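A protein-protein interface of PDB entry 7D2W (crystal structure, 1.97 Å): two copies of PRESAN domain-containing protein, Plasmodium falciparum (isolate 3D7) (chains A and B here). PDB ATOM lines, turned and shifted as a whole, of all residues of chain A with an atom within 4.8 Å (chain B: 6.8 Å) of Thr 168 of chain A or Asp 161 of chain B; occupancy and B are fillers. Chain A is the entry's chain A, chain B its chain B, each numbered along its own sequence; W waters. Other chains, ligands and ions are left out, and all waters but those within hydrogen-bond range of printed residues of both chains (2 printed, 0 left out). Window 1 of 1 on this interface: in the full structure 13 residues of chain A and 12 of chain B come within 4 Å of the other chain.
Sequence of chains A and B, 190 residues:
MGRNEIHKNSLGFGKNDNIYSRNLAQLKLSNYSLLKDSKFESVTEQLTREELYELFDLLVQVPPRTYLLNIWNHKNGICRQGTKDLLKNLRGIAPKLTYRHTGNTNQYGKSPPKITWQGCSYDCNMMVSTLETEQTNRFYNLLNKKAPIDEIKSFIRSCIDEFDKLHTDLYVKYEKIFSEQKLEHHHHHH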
ATOM      1  N   ASP A 164      18.815   3.263  11.273  1.00  0.00           N
ATOM      2  CA  ASP A 164      20.059   3.369  12.021  1.00  0.00           C
ATOM      3  C   ASP A 164      20.309   4.810  12.459  1.00  0.00           C
ATOM      4  O   ASP A 164      20.785   5.051  13.576  1.00  0.00           O
ATOM      5  CB  ASP A 164      21.233   2.862  11.186  1.00  0.00           C
ATOM      6  CG  ASP A 164      21.219   1.355  11.003  1.00  0.00           C
ATOM      7  OD1 ASP A 164      20.461   0.646  11.727  1.00  0.00           O
ATOM      8  OD2 ASP A 164      21.981   0.883  10.128  1.00  0.00           O
ATOM      9  N   LYS A 165      19.993   5.774  11.594  1.00  0.00           N
ATOM     10  CA  LYS A 165      20.173   7.175  11.975  1.00  0.00           C
ATOM     11  C   LYS A 165      19.196   7.572  13.070  1.00  0.00           C
ATOM     12  O   LYS A 165      19.565   8.298  13.998  1.00  0.00           O
ATOM     13  CB  LYS A 165      20.023   8.103  10.770  1.00  0.00           C
ATOM     14  CG  LYS A 165      19.895   9.599  11.184  1.00  0.00           C
ATOM     15  CD  LYS A 165      20.739  10.544  10.365  1.00  0.00           C
ATOM     16  CE  LYS A 165      20.624  11.994  10.889  1.00  0.00           C
ATOM     17  NZ  LYS A 165      21.271  12.253  12.236  1.00  0.00           N
ATOM     18  N   LEU A 166      17.949   7.100  12.994  1.00  0.00           N
ATOM     19  CA  LEU A 166      17.003   7.405  14.065  1.00  0.00           C
ATOM     20  C   LEU A 166      17.476   6.808  15.386  1.00  0.00           C
ATOM     21  O   LEU A 166      17.442   7.480  16.423  1.00  0.00           O
ATOM     22  CB  LEU A 166      15.597   6.904  13.708  1.00  0.00           C
ATOM     23  CG  LEU A 166      14.571   6.993  14.845  1.00  0.00           C
ATOM     24  CD1 LEU A 166      14.371   8.418  15.284  1.00  0.00           C
ATOM     25  CD2 LEU A 166      13.236   6.372  14.432  1.00  0.00           C
ATOM     26  N   HIS A 167      17.936   5.552  15.370  1.00  0.00           N
ATOM     27  CA  HIS A 167      18.430   4.941  16.603  1.00  0.00           C
ATOM     28  C   HIS A 167      19.629   5.710  17.150  1.00  0.00           C
ATOM     29  O   HIS A 167      19.790   5.852  18.368  1.00  0.00           O
ATOM     30  CB  HIS A 167      18.804   3.479  16.357  1.00  0.00           C
ATOM     31  CG  HIS A 167      17.624   2.577  16.155  1.00  0.00           C
ATOM     32  ND1 HIS A 167      17.688   1.437  15.386  1.00  0.00           N
ATOM     33  CD2 HIS A 167      16.358   2.644  16.628  1.00  0.00           C
ATOM     34  CE1 HIS A 167      16.508   0.839  15.391  1.00  0.00           C
ATOM     35  NE2 HIS A 167      15.684   1.553  16.135  1.00  0.00           N
ATOM     36  N   THR A 168      20.483   6.206  16.262  1.00  0.00           N
ATOM     37  CA  THR A 168      21.608   7.030  16.690  1.00  0.00           C
ATOM     38  C   THR A 168      21.117   8.338  17.297  1.00  0.00           C
ATOM     39  O   THR A 168      21.583   8.747  18.367  1.00  0.00           O
ATOM     40  CB  THR A 168      22.533   7.302  15.503  1.00  0.00           C
ATOM     41  OG1 THR A 168      23.018   6.057  14.997  1.00  0.00           O
ATOM     42  CG2 THR A 168      23.736   8.170  15.923  1.00  0.00           C
ATOM     43  N   ASP A 169      20.173   9.004  16.623  1.00  0.00           N
ATOM     44  CA  ASP A 169      19.640  10.263  17.132  1.00  0.00           C
ATOM     45  C   ASP A 169      19.057  10.093  18.526  1.00  0.00           C
ATOM     46  O   ASP A 169      19.293  10.924  19.416  1.00  0.00           O
ATOM     47  CB  ASP A 169      18.578  10.810  16.180  1.00  0.00           C
ATOM     48  CG  ASP A 169      19.172  11.402  14.923  1.00  0.00           C
ATOM     49  OD1 ASP A 169      20.412  11.437  14.803  1.00  0.00           O
ATOM     50  OD2 ASP A 169      18.396  11.803  14.039  1.00  0.00           O
ATOM     51  N   LEU A 170      18.276   9.027  18.731  1.00  0.00           N
ATOM     52  CA  LEU A 170      17.675   8.789  20.039  1.00  0.00           C
ATOM     53  C   LEU A 170      18.736   8.493  21.095  1.00  0.00           C
ATOM     54  O   LEU A 170      18.655   8.991  22.221  1.00  0.00           O
ATOM     55  CB  LEU A 170      16.675   7.629  19.943  1.00  0.00           C
ATOM     56  CG  LEU A 170      15.379   7.941  19.183  1.00  0.00           C
ATOM     57  CD1 LEU A 170      14.580   6.649  18.905  1.00  0.00           C
ATOM     58  CD2 LEU A 170      14.546   8.919  19.988  1.00  0.00           C
ATOM     59  N   TYR A 171      19.728   7.667  20.766  1.00  0.00           N
ATOM     60  CA  TYR A 171      20.761   7.361  21.749  1.00  0.00           C
ATOM     61  C   TYR A 171      21.519   8.624  22.163  1.00  0.00           C
ATOM     62  O   TYR A 171      21.726   8.857  23.357  1.00  0.00           O
ATOM     63  CB  TYR A 171      21.727   6.291  21.223  1.00  0.00           C
ATOM     64  CG  TYR A 171      22.598   5.705  22.326  1.00  0.00           C
ATOM     65  CD1 TYR A 171      22.103   4.738  23.190  1.00  0.00           C
ATOM     66  CD2 TYR A 171      23.903   6.142  22.518  1.00  0.00           C
ATOM     67  CE1 TYR A 171      22.885   4.219  24.207  1.00  0.00           C
ATOM     68  CE2 TYR A 171      24.693   5.629  23.533  1.00  0.00           C
ATOM     69  CZ  TYR A 171      24.180   4.667  24.373  1.00  0.00           C
ATOM     70  OH  TYR A 171      24.961   4.149  25.382  1.00  0.00           O
ATOM     71  N   VAL A 172      21.917   9.447  21.195  1.00  0.00           N
ATOM     72  CA  VAL A 172      22.626  10.691  21.480  1.00  0.00           C
ATOM     73  C   VAL A 172      21.784  11.588  22.382  1.00  0.00           C
ATOM     74  O   VAL A 172      22.269  12.122  23.390  1.00  0.00           O
ATOM     75  CB  VAL A 172      22.989  11.382  20.150  1.00  0.00           C
ATOM     76  CG1 VAL A 172      23.250  12.867  20.329  1.00  0.00           C
ATOM     77  CG2 VAL A 172      24.195  10.678  19.514  1.00  0.00           C
ATOM     78  N   ARG B  49      25.212  19.261   6.319  1.00  0.00           N
ATOM     79  CA  ARG B  49      24.724  17.903   6.505  1.00  0.00           C
ATOM     80  C   ARG B  49      23.500  17.631   5.642  1.00  0.00           C
ATOM     81  O   ARG B  49      23.407  16.601   4.961  1.00  0.00           O
ATOM     82  CB  ARG B  49      24.407  17.706   7.987  1.00  0.00           C
ATOM     83  CG  ARG B  49      24.263  16.284   8.441  1.00  0.00           C
ATOM     84  CD  ARG B  49      23.903  16.287   9.918  1.00  0.00           C
ATOM     85  NE  ARG B  49      25.082  16.340  10.779  1.00  0.00           N
ATOM     86  CZ  ARG B  49      25.461  15.337  11.575  1.00  0.00           C
ATOM     87  NH1 ARG B  49      24.753  14.218  11.617  1.00  0.00           N
ATOM     88  NH2 ARG B  49      26.536  15.460  12.346  1.00  0.00           N
ATOM     89  N   TYR B  53      23.226  14.826   2.633  1.00  0.00           N
ATOM     90  CA  TYR B  53      22.221  13.765   2.590  1.00  0.00           C
ATOM     91  C   TYR B  53      21.404  13.832   1.304  1.00  0.00           C
ATOM     92  O   TYR B  53      21.030  12.798   0.739  1.00  0.00           O
ATOM     93  CB  TYR B  53      21.303  13.861   3.811  1.00  0.00           C
ATOM     94  CG  TYR B  53      21.937  13.422   5.120  1.00  0.00           C
ATOM     95  CD1 TYR B  53      22.863  12.392   5.159  1.00  0.00           C
ATOM     96  CD2 TYR B  53      21.587  14.036   6.321  1.00  0.00           C
ATOM     97  CE1 TYR B  53      23.436  11.984   6.361  1.00  0.00           C
ATOM     98  CE2 TYR B  53      22.152  13.638   7.528  1.00  0.00           C
ATOM     99  CZ  TYR B  53      23.076  12.614   7.544  1.00  0.00           C
ATOM    100  OH  TYR B  53      23.632  12.225   8.748  1.00  0.00           O
ATOM    101  N   CYS B  79      32.078  16.489   9.966  1.00  0.00           N
ATOM    102  CA  CYS B  79      32.517  15.912  11.233  1.00  0.00           C
ATOM    103  C   CYS B  79      33.496  16.838  11.955  1.00  0.00           C
ATOM    104  O   CYS B  79      33.494  16.898  13.191  1.00  0.00           O
ATOM    105  CB  CYS B  79      33.129  14.523  11.004  1.00  0.00           C
ATOM    106  SG  CYS B  79      31.926  13.278  10.314  1.00  0.00           S
ATOM    107  N   GLN B 135      38.263   5.761   9.528  1.00  0.00           N
ATOM    108  CA  GLN B 135      37.138   5.749   8.598  1.00  0.00           C
ATOM    109  C   GLN B 135      37.608   5.975   7.162  1.00  0.00           C
ATOM    110  O   GLN B 135      37.132   5.310   6.235  1.00  0.00           O
ATOM    111  CB  GLN B 135      36.109   6.797   9.014  1.00  0.00           C
ATOM    112  CG  GLN B 135      35.333   6.412  10.277  1.00  0.00           C
ATOM    113  CD  GLN B 135      34.302   7.476  10.607  1.00  0.00           C
ATOM    114  OE1 GLN B 135      34.372   8.587  10.082  1.00  0.00           O
ATOM    115  NE2 GLN B 135      33.341   7.146  11.472  1.00  0.00           N
ATOM    116  N   SER B 154      25.516   3.502   2.511  1.00  0.00           N
ATOM    117  CA  SER B 154      25.343   3.038   3.889  1.00  0.00           C
ATOM    118  C   SER B 154      26.591   3.311   4.718  1.00  0.00           C
ATOM    119  O   SER B 154      26.501   3.746   5.871  1.00  0.00           O
ATOM    120  CB  SER B 154      25.030   1.531   3.919  1.00  0.00           C
ATOM    121  OG  SER B 154      23.754   1.243   3.381  1.00  0.00           O
ATOM    122  N   ILE B 156      29.000   5.625   4.339  1.00  0.00           N
ATOM    123  CA  ILE B 156      29.229   7.030   4.661  1.00  0.00           C
ATOM    124  C   ILE B 156      28.233   7.497   5.706  1.00  0.00           C
ATOM    125  O   ILE B 156      28.604   8.175   6.672  1.00  0.00           O
ATOM    126  CB  ILE B 156      29.174   7.917   3.405  1.00  0.00           C
ATOM    127  CG1 ILE B 156      30.233   7.480   2.409  1.00  0.00           C
ATOM    128  CG2 ILE B 156      29.387   9.402   3.805  1.00  0.00           C
ATOM    129  CD1 ILE B 156      30.183   8.276   1.106  1.00  0.00           C
ATOM    130  N   ARG B 157      26.959   7.120   5.542  1.00  0.00           N
ATOM    131  CA  ARG B 157      25.955   7.445   6.550  1.00  0.00           C
ATOM    132  C   ARG B 157      26.349   6.888   7.912  1.00  0.00           C
ATOM    133  O   ARG B 157      26.273   7.589   8.926  1.00  0.00           O
ATOM    134  CB  ARG B 157      24.593   6.894   6.124  1.00  0.00           C
ATOM    135  CG  ARG B 157      23.907   7.657   4.994  1.00  0.00           C
ATOM    136  CD  ARG B 157      22.796   6.808   4.385  1.00  0.00           C
ATOM    137  NE  ARG B 157      22.004   7.580   3.441  1.00  0.00           N
ATOM    138  CZ  ARG B 157      21.358   7.074   2.396  1.00  0.00           C
ATOM    139  NH1 ARG B 157      21.374   5.760   2.142  1.00  0.00           N
ATOM    140  NH2 ARG B 157      20.672   7.895   1.611  1.00  0.00           N
ATOM    141  N   SER B 158      26.817   5.640   7.947  1.00  0.00           N
ATOM    142  CA  SER B 158      27.193   5.033   9.221  1.00  0.00           C
ATOM    143  C   SER B 158      28.399   5.724   9.853  1.00  0.00           C
ATOM    144  O   SER B 158      28.507   5.771  11.086  1.00  0.00           O
ATOM    145  CB  SER B 158      27.469   3.536   9.024  1.00  0.00           C
ATOM    146  OG  SER B 158      28.785   3.328   8.532  1.00  0.00           O
ATOM    147  N   CYS B 159      29.329   6.224   9.038  1.00  0.00           N
ATOM    148  CA  CYS B 159      30.481   6.951   9.565  1.00  0.00           C
ATOM    149  C   CYS B 159      30.068   8.253  10.237  1.00  0.00           C
ATOM    150  O   CYS B 159      30.679   8.675  11.226  1.00  0.00           O
ATOM    151  CB  CYS B 159      31.472   7.249   8.436  1.00  0.00           C
ATOM    152  SG  CYS B 159      32.452   5.824   7.917  1.00  0.00           S
ATOM    153  N   ILE B 160      29.070   8.931   9.685  1.00  0.00           N
ATOM    154  CA  ILE B 160      28.581  10.153  10.313  1.00  0.00           C
ATOM    155  C   ILE B 160      27.865   9.827  11.622  1.00  0.00           C
ATOM    156  O   ILE B 160      28.030  10.542  12.619  1.00  0.00           O
ATOM    157  CB  ILE B 160      27.691  10.926   9.320  1.00  0.00           C
ATOM    158  CG1 ILE B 160      28.551  11.410   8.147  1.00  0.00           C
ATOM    159  CG2 ILE B 160      27.009  12.132   9.999  1.00  0.00           C
ATOM    160  CD1 ILE B 160      27.742  11.990   6.981  1.00  0.00           C
ATOM    161  N   ASP B 161      27.080   8.736  11.653  1.00  0.00           N
ATOM    162  CA  ASP B 161      26.482   8.293  12.916  1.00  0.00           C
ATOM    163  C   ASP B 161      27.562   7.985  13.952  1.00  0.00           C
ATOM    164  O   ASP B 161      27.417   8.324  15.134  1.00  0.00           O
ATOM    165  CB  ASP B 161      25.625   7.032  12.718  1.00  0.00           C
ATOM    166  CG  ASP B 161      24.377   7.266  11.869  1.00  0.00           C
ATOM    167  OD1 ASP B 161      23.990   8.426  11.644  1.00  0.00           O
ATOM    168  OD2 ASP B 161      23.783   6.257  11.405  1.00  0.00           O
ATOM    169  N   GLU B 162      28.624   7.283  13.536  1.00  0.00           N
ATOM    170  CA  GLU B 162      29.700   6.922  14.458  1.00  0.00           C
ATOM    171  C   GLU B 162      30.372   8.167  15.040  1.00  0.00           C
ATOM    172  O   GLU B 162      30.739   8.201  16.228  1.00  0.00           O
ATOM    173  CB  GLU B 162      30.718   6.039  13.723  1.00  0.00           C
ATOM    174  CG  GLU B 162      31.622   5.227  14.608  1.00  0.00           C
ATOM    175  CD  GLU B 162      32.671   4.449  13.816  1.00  0.00           C
ATOM    176  OE1 GLU B 162      32.646   4.474  12.549  1.00  0.00           O
ATOM    177  OE2 GLU B 162      33.544   3.843  14.469  1.00  0.00           O
ATOM    178  N   PHE B 163      30.556   9.196  14.212  1.00  0.00           N
ATOM    179  CA  PHE B 163      31.153  10.441  14.695  1.00  0.00           C
ATOM    180  C   PHE B 163      30.227  11.180  15.654  1.00  0.00           C
ATOM    181  O   PHE B 163      30.690  11.725  16.666  1.00  0.00           O
ATOM    182  CB  PHE B 163      31.543  11.335  13.513  1.00  0.00           C
ATOM    183  CG  PHE B 163      33.013  11.356  13.267  1.00  0.00           C
ATOM    184  CD1 PHE B 163      33.857  11.997  14.163  1.00  0.00           C
ATOM    185  CD2 PHE B 163      33.563  10.695  12.180  1.00  0.00           C
ATOM    186  CE1 PHE B 163      35.223  12.013  13.949  1.00  0.00           C
ATOM    187  CE2 PHE B 163      34.923  10.701  11.966  1.00  0.00           C
ATOM    188  CZ  PHE B 163      35.753  11.339  12.850  1.00  0.00           C
ATOM    189  N   ASP B 164      28.921  11.216  15.356  1.00  0.00           N
ATOM    190  CA  ASP B 164      27.964  11.795  16.298  1.00  0.00           C
ATOM    191  C   ASP B 164      28.021  11.084  17.648  1.00  0.00           C
ATOM    192  O   ASP B 164      27.976  11.729  18.704  1.00  0.00           O
ATOM    193  CB  ASP B 164      26.540  11.730  15.736  1.00  0.00           C
ATOM    194  CG  ASP B 164      26.326  12.647  14.537  1.00  0.00           C
ATOM    195  OD1 ASP B 164      27.183  13.516  14.261  1.00  0.00           O
ATOM    196  OD2 ASP B 164      25.276  12.507  13.871  1.00  0.00           O
ATOM    197  N   LYS B 165      28.111   9.749  17.634  1.00  0.00           N
ATOM    198  CA  LYS B 165      28.206   9.005  18.890  1.00  0.00           C
ATOM    199  C   LYS B 165      29.501   9.324  19.633  1.00  0.00           C
ATOM    200  O   LYS B 165      29.506   9.446  20.865  1.00  0.00           O
ATOM    201  CB  LYS B 165      28.106   7.494  18.627  1.00  0.00           C
ATOM    202  CG  LYS B 165      26.697   6.988  18.312  1.00  0.00           C
ATOM    203  CD  LYS B 165      26.539   5.514  18.707  1.00  0.00           C
ATOM    204  CE  LYS B 165      25.104   5.022  18.510  1.00  0.00           C
ATOM    205  NZ  LYS B 165      24.740   3.899  19.435  1.00  0.00           N
ATOM    206  N   LEU B 166      30.616   9.434  18.908  1.00  0.00           N
ATOM    207  CA  LEU B 166      31.886   9.732  19.564  1.00  0.00           C
ATOM    208  C   LEU B 166      31.840  11.115  20.195  1.00  0.00           C
ATOM    209  O   LEU B 166      32.232  11.296  21.354  1.00  0.00           O
ATOM    210  CB  LEU B 166      33.053   9.637  18.573  1.00  0.00           C
ATOM    211  CG  LEU B 166      34.400  10.111  19.148  1.00  0.00           C
ATOM    212  CD1 LEU B 166      34.846   9.231  20.295  1.00  0.00           C
ATOM    213  CD2 LEU B 166      35.489  10.174  18.079  1.00  0.00           C
HETATM  214  O   HOH W   1      22.743  11.781  15.808  1.00  0.00           O
HETATM  215  O   HOH W   2      23.910  10.844  12.299  1.00  0.00           O
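The side-chain hydroxyl (OG1) of Thr 168 of chain A is in hydrogen-bond range of the backbone carbonyl oxygen (O) of Asp 164 of chain A, 2.8 Å away.
The side-chain carboxylate (OD1) of Asp 169 of chain A is in salt-bridge range of the side-chain amino group (NZ) of Lys 165 of chain A (2.8 Å).
Among the printed residues, pairs that only touch across the chains: Asp 164 of chain A with Asp 161 of chain B, Lys 165 of chain A with Tyr 53 of chain B, Lys 165 of chain A with Asp 161 of chain B, Thr 168 of chain A with Asp 161 of chain B, Thr 168 of chain A with Lys 165 of chain B and Tyr 171 of chain A with Lys 165 of chain B.
Printed residues of chain B within 4 Å of Asp 164 of chain A: Asp 161.
Printed residues of chain B within 4 Å of Thr 168 of chain A: Asp 161 and Lys 165.
Of the printed residues of chain B, Tyr 171 of chain A touches Lys 165.
Of chain A, only Asp 164, Lys 165 and Thr 168 come within 4 Å of Asp 161 of chain B.
Phe 163 of chain B touches none of the printed residues of chain A.
Of the printed residues of chain A, Lys 165 of chain B touches Thr 168 (3.98 Å) and Tyr 171 (3.9 Å).
The nearest printed residue of chain A that does not touch Tyr 53 of chain B is Asp 169 of chain A (6.9 Å).
Of the 16 printed residues of chain B, 3 touch a printed residue of chain A.
Hydrophobic or aromatic side chains of chain A within 4 Å of the printed part of chain B: Tyr 171.
Positions printed for both chains: 164, 165 and 166.
Water W2 lies within hydrogen-bond range of the side-chain carboxylate (OD1) of Asp 161 of chain B (2.5 Å), the side-chain carboxylate (OD2) of Asp 164 of chain B (2.7 Å) and the side-chain amino group (NZ) of Lys 165 of chain A (3.0 Å).
Water W1 bridges OD1 of Asp 169 of chain A (2.6 Å) and OD2 of Asp 164 of chain B (3.3 Å).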
